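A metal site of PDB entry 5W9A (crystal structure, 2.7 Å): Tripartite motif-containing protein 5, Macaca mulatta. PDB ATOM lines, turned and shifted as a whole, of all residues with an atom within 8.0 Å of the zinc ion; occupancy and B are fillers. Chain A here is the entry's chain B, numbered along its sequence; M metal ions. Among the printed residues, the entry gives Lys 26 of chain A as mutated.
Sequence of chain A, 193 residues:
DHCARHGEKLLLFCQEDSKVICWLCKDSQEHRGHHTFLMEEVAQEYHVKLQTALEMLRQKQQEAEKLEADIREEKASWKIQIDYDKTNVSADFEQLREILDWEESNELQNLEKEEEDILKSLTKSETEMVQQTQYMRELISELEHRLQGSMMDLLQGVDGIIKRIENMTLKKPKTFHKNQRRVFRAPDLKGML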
ATOM      1  N   HIS A   2     -14.380  -8.864  21.833  1.00  0.00           N
ATOM      2  CA  HIS A   2     -13.982  -7.497  22.122  1.00  0.00           C
ATOM      3  C   HIS A   2     -12.571  -7.452  22.678  1.00  0.00           C
ATOM      4  O   HIS A   2     -12.014  -8.457  23.127  1.00  0.00           O
ATOM      5  CB  HIS A   2     -14.964  -6.850  23.114  1.00  0.00           C
ATOM      6  CG  HIS A   2     -16.320  -6.581  22.540  1.00  0.00           C
ATOM      7  ND1 HIS A   2     -17.339  -6.014  23.270  1.00  0.00           N
ATOM      8  CD2 HIS A   2     -16.825  -6.814  21.302  1.00  0.00           C
ATOM      9  CE1 HIS A   2     -18.412  -5.906  22.507  1.00  0.00           C
ATOM     10  NE2 HIS A   2     -18.134  -6.383  21.312  1.00  0.00           N
ATOM     11  N   CYS A   3     -11.977  -6.260  22.635  1.00  0.00           N
ATOM     12  CA  CYS A   3     -10.589  -6.088  23.012  1.00  0.00           C
ATOM     13  C   CYS A   3     -10.429  -6.131  24.526  1.00  0.00           C
ATOM     14  O   CYS A   3     -11.290  -5.642  25.272  1.00  0.00           O
ATOM     15  CB  CYS A   3     -10.039  -4.776  22.470  1.00  0.00           C
ATOM     16  SG  CYS A   3      -8.290  -4.483  22.818  1.00  0.00           S
ATOM     17  N   ALA A   4      -9.328  -6.723  24.983  1.00  0.00           N
ATOM     18  CA  ALA A   4      -9.047  -6.770  26.411  1.00  0.00           C
ATOM     19  C   ALA A   4      -8.424  -5.476  26.906  1.00  0.00           C
ATOM     20  O   ALA A   4      -8.626  -5.090  28.061  1.00  0.00           O
ATOM     21  CB  ALA A   4      -8.128  -7.951  26.729  1.00  0.00           C
ATOM     22  N   ARG A   5      -7.655  -4.789  26.054  1.00  0.00           N
ATOM     23  CA  ARG A   5      -6.972  -3.572  26.473  1.00  0.00           C
ATOM     24  C   ARG A   5      -7.900  -2.361  26.454  1.00  0.00           C
ATOM     25  O   ARG A   5      -7.848  -1.528  27.369  1.00  0.00           O
ATOM     26  CB  ARG A   5      -5.753  -3.326  25.579  1.00  0.00           C
ATOM     27  CG  ARG A   5      -4.917  -2.123  25.972  1.00  0.00           C
ATOM     28  CD  ARG A   5      -3.758  -1.908  24.994  1.00  0.00           C
ATOM     29  NE  ARG A   5      -2.810  -3.016  25.010  1.00  0.00           N
ATOM     30  CZ  ARG A   5      -2.737  -3.956  24.073  1.00  0.00           C
ATOM     31  NH1 ARG A   5      -3.560  -3.929  23.034  1.00  0.00           N
ATOM     32  NH2 ARG A   5      -1.839  -4.921  24.162  1.00  0.00           N
ATOM     33  N   HIS A   6      -8.751  -2.247  25.438  1.00  0.00           N
ATOM     34  CA  HIS A   6      -9.618  -1.081  25.283  1.00  0.00           C
ATOM     35  C   HIS A   6     -11.103  -1.412  25.403  1.00  0.00           C
ATOM     36  O   HIS A   6     -11.845  -0.626  25.992  1.00  0.00           O
ATOM     37  CB  HIS A   6      -9.363  -0.415  23.930  1.00  0.00           C
ATOM     38  CG  HIS A   6      -8.003   0.201  23.807  1.00  0.00           C
ATOM     39  ND1 HIS A   6      -6.925  -0.482  23.290  1.00  0.00           N
ATOM     40  CD2 HIS A   6      -7.538   1.427  24.149  1.00  0.00           C
ATOM     41  CE1 HIS A   6      -5.854   0.300  23.306  1.00  0.00           C
ATOM     42  NE2 HIS A   6      -6.203   1.464  23.822  1.00  0.00           N
ATOM     43  N   GLY A   7     -11.549  -2.540  24.861  1.00  0.00           N
ATOM     44  CA  GLY A   7     -12.943  -2.930  24.934  1.00  0.00           C
ATOM     45  C   GLY A   7     -13.703  -2.866  23.628  1.00  0.00           C
ATOM     46  O   GLY A   7     -14.878  -3.230  23.603  1.00  0.00           O
ATOM     47  N   GLU A   8     -13.074  -2.398  22.546  1.00  0.00           N
ATOM     48  CA  GLU A   8     -13.734  -2.312  21.248  1.00  0.00           C
ATOM     49  C   GLU A   8     -13.552  -3.604  20.454  1.00  0.00           C
ATOM     50  O   GLU A   8     -12.772  -4.485  20.821  1.00  0.00           O
ATOM     51  CB  GLU A   8     -13.197  -1.116  20.471  1.00  0.00           C
ATOM     52  CG  GLU A   8     -13.521   0.236  21.090  1.00  0.00           C
ATOM     53  CD  GLU A   8     -14.967   0.638  20.884  1.00  0.00           C
ATOM     54  OE1 GLU A   8     -15.621   0.075  19.981  1.00  0.00           O
ATOM     55  OE2 GLU A   8     -15.445   1.511  21.629  1.00  0.00           O
ATOM     56  N   LYS A   9     -14.297  -3.713  19.362  1.00  0.00           N
ATOM     57  CA  LYS A   9     -14.228  -4.895  18.526  1.00  0.00           C
ATOM     58  C   LYS A   9     -12.861  -5.008  17.850  1.00  0.00           C
ATOM     59  O   LYS A   9     -12.197  -4.000  17.580  1.00  0.00           O
ATOM     60  CB  LYS A   9     -15.317  -4.846  17.449  1.00  0.00           C
ATOM     61  CG  LYS A   9     -16.729  -4.675  17.998  1.00  0.00           C
ATOM     62  CD  LYS A   9     -17.731  -4.538  16.866  1.00  0.00           C
ATOM     63  CE  LYS A   9     -19.134  -4.292  17.392  1.00  0.00           C
ATOM     64  NZ  LYS A   9     -20.120  -4.104  16.284  1.00  0.00           N
ATOM     65  N   LEU A  10     -12.446  -6.244  17.584  1.00  0.00           N
ATOM     66  CA  LEU A  10     -11.213  -6.509  16.839  1.00  0.00           C
ATOM     67  C   LEU A  10     -11.609  -6.789  15.392  1.00  0.00           C
ATOM     68  O   LEU A  10     -11.792  -7.936  14.997  1.00  0.00           O
ATOM     69  CB  LEU A  10     -10.428  -7.667  17.446  1.00  0.00           C
ATOM     70  CG  LEU A  10      -9.907  -7.493  18.872  1.00  0.00           C
ATOM     71  CD1 LEU A  10     -10.882  -8.093  19.861  1.00  0.00           C
ATOM     72  CD2 LEU A  10      -8.534  -8.138  19.026  1.00  0.00           C
ATOM     73  N   VAL A  20      -4.425  -8.578  15.311  1.00  0.00           N
ATOM     74  CA  VAL A  20      -5.718  -7.929  15.147  1.00  0.00           C
ATOM     75  C   VAL A  20      -5.963  -7.008  16.339  1.00  0.00           C
ATOM     76  O   VAL A  20      -5.687  -7.370  17.489  1.00  0.00           O
ATOM     77  CB  VAL A  20      -6.835  -8.972  14.986  1.00  0.00           C
ATOM     78  CG1 VAL A  20      -6.667  -9.722  13.671  1.00  0.00           C
ATOM     79  CG2 VAL A  20      -6.849  -9.939  16.160  1.00  0.00           C
ATOM     80  N   ILE A  21      -6.462  -5.808  16.056  1.00  0.00           N
ATOM     81  CA  ILE A  21      -6.652  -4.795  17.096  1.00  0.00           C
ATOM     82  C   ILE A  21      -7.964  -4.058  16.863  1.00  0.00           C
ATOM     83  O   ILE A  21      -8.768  -4.434  16.012  1.00  0.00           O
ATOM     84  CB  ILE A  21      -5.472  -3.796  17.108  1.00  0.00           C
ATOM     85  CG1 ILE A  21      -5.210  -3.262  15.700  1.00  0.00           C
ATOM     86  CG2 ILE A  21      -4.217  -4.444  17.678  1.00  0.00           C
ATOM     87  CD1 ILE A  21      -4.099  -2.236  15.627  1.00  0.00           C
ATOM     88  N   CYS A  22      -8.184  -2.996  17.640  1.00  0.00           N
ATOM     89  CA  CYS A  22      -9.327  -2.122  17.499  1.00  0.00           C
ATOM     90  C   CYS A  22      -8.863  -0.754  16.998  1.00  0.00           C
ATOM     91  O   CYS A  22      -7.684  -0.528  16.743  1.00  0.00           O
ATOM     92  CB  CYS A  22     -10.072  -1.985  18.829  1.00  0.00           C
ATOM     93  SG  CYS A  22      -9.252  -0.947  20.053  1.00  0.00           S
ATOM     94  N   TRP A  23      -9.821   0.161  16.836  1.00  0.00           N
ATOM     95  CA  TRP A  23      -9.480   1.494  16.357  1.00  0.00           C
ATOM     96  C   TRP A  23      -8.748   2.309  17.422  1.00  0.00           C
ATOM     97  O   TRP A  23      -7.959   3.193  17.085  1.00  0.00           O
ATOM     98  CB  TRP A  23     -10.723   2.226  15.872  1.00  0.00           C
ATOM     99  CG  TRP A  23     -11.752   2.471  16.943  1.00  0.00           C
ATOM    100  CD1 TRP A  23     -12.633   1.566  17.445  1.00  0.00           C
ATOM    101  CD2 TRP A  23     -11.991   3.707  17.628  1.00  0.00           C
ATOM    102  NE1 TRP A  23     -13.416   2.163  18.413  1.00  0.00           N
ATOM    103  CE2 TRP A  23     -13.035   3.473  18.540  1.00  0.00           C
ATOM    104  CE3 TRP A  23     -11.419   4.976  17.565  1.00  0.00           C
ATOM    105  CZ2 TRP A  23     -13.535   4.465  19.379  1.00  0.00           C
ATOM    106  CZ3 TRP A  23     -11.912   5.964  18.397  1.00  0.00           C
ATOM    107  CH2 TRP A  23     -12.960   5.708  19.291  1.00  0.00           C
ATOM    108  N   LEU A  24      -9.022   2.043  18.702  1.00  0.00           N
ATOM    109  CA  LEU A  24      -8.302   2.733  19.761  1.00  0.00           C
ATOM    110  C   LEU A  24      -6.840   2.313  19.808  1.00  0.00           C
ATOM    111  O   LEU A  24      -5.976   3.117  20.183  1.00  0.00           O
ATOM    112  CB  LEU A  24      -8.973   2.483  21.115  1.00  0.00           C
ATOM    113  CG  LEU A  24     -10.311   3.192  21.343  1.00  0.00           C
ATOM    114  CD1 LEU A  24     -10.926   2.775  22.672  1.00  0.00           C
ATOM    115  CD2 LEU A  24     -10.122   4.698  21.287  1.00  0.00           C
ATOM    116  N   CYS A  25      -6.535   1.058  19.453  1.00  0.00           N
ATOM    117  CA  CYS A  25      -5.151   0.619  19.394  1.00  0.00           C
ATOM    118  C   CYS A  25      -4.398   1.274  18.240  1.00  0.00           C
ATOM    119  O   CYS A  25      -3.167   1.338  18.279  1.00  0.00           O
ATOM    120  CB  CYS A  25      -5.086  -0.902  19.250  1.00  0.00           C
ATOM    121  SG  CYS A  25      -5.836  -1.824  20.609  1.00  0.00           S
ATOM    122  N   LYS A  26      -5.105   1.752  17.218  1.00  0.00           N
ATOM    123  CA  LYS A  26      -4.440   2.394  16.087  1.00  0.00           C
ATOM    124  C   LYS A  26      -3.889   3.762  16.454  1.00  0.00           C
ATOM    125  O   LYS A  26      -2.831   4.154  15.950  1.00  0.00           O
ATOM    126  CB  LYS A  26      -5.410   2.505  14.912  1.00  0.00           C
ATOM    127  CG  LYS A  26      -4.771   3.008  13.621  1.00  0.00           C
ATOM    128  CD  LYS A  26      -5.796   3.031  12.483  1.00  0.00           C
ATOM    129  CE  LYS A  26      -6.903   4.036  12.756  1.00  0.00           C
ATOM    130  NZ  LYS A  26      -7.868   4.130  11.622  1.00  0.00           N
ATOM    131  N   SER A  28      -3.177   4.748  19.689  1.00  0.00           N
ATOM    132  CA  SER A  28      -2.304   4.675  20.850  1.00  0.00           C
ATOM    133  C   SER A  28      -0.842   4.507  20.409  1.00  0.00           C
ATOM    134  O   SER A  28      -0.543   4.245  19.241  1.00  0.00           O
ATOM    135  CB  SER A  28      -2.714   3.538  21.775  1.00  0.00           C
ATOM    136  OG  SER A  28      -2.540   2.282  21.151  1.00  0.00           O
ATOM    137  N   HIS A  31       0.545   0.918  18.609  1.00  0.00           N
ATOM    138  CA  HIS A  31       0.499   0.702  17.159  1.00  0.00           C
ATOM    139  C   HIS A  31       0.517   2.025  16.391  1.00  0.00           C
ATOM    140  O   HIS A  31      -0.063   2.126  15.315  1.00  0.00           O
ATOM    141  CB  HIS A  31      -0.727  -0.119  16.778  1.00  0.00           C
ATOM    142  CG  HIS A  31      -0.861  -1.403  17.544  1.00  0.00           C
ATOM    143  ND1 HIS A  31      -0.141  -2.540  17.231  1.00  0.00           N
ATOM    144  CD2 HIS A  31      -1.625  -1.726  18.616  1.00  0.00           C
ATOM    145  CE1 HIS A  31      -0.460  -3.508  18.070  1.00  0.00           C
ATOM    146  NE2 HIS A  31      -1.359  -3.038  18.924  1.00  0.00           N
HETATM  147 ZN    ZN M   1      -8.091  -2.152  21.769  1.00  0.00          ZN
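The zinc ion is bound by SG of Cys 22, ND1 of His 6, SG of Cys 25 and SG of Cys 3.
The side-chain sulfur (SG) of Cys 3 sits close to the backbone NH (N) of Arg 5 (3.3 Å).
The side-chain sulfur of Cys 22 sits close to the backbone NH of Leu 24, 3.3 Å away.
OG of Ser 28 sits at hydrogen-bond distance from O of Cys 25 (3.1 Å).
O of Glu 8 is in hydrogen-bond range of N of Cys 3 (2.7 Å).
Within 4 Å of the zinc ion: Cys 3, His 6, Cys 22 and Cys 25.
The nearest printed residue that does not touch the zinc ion is Arg 5 (4.6 Å).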
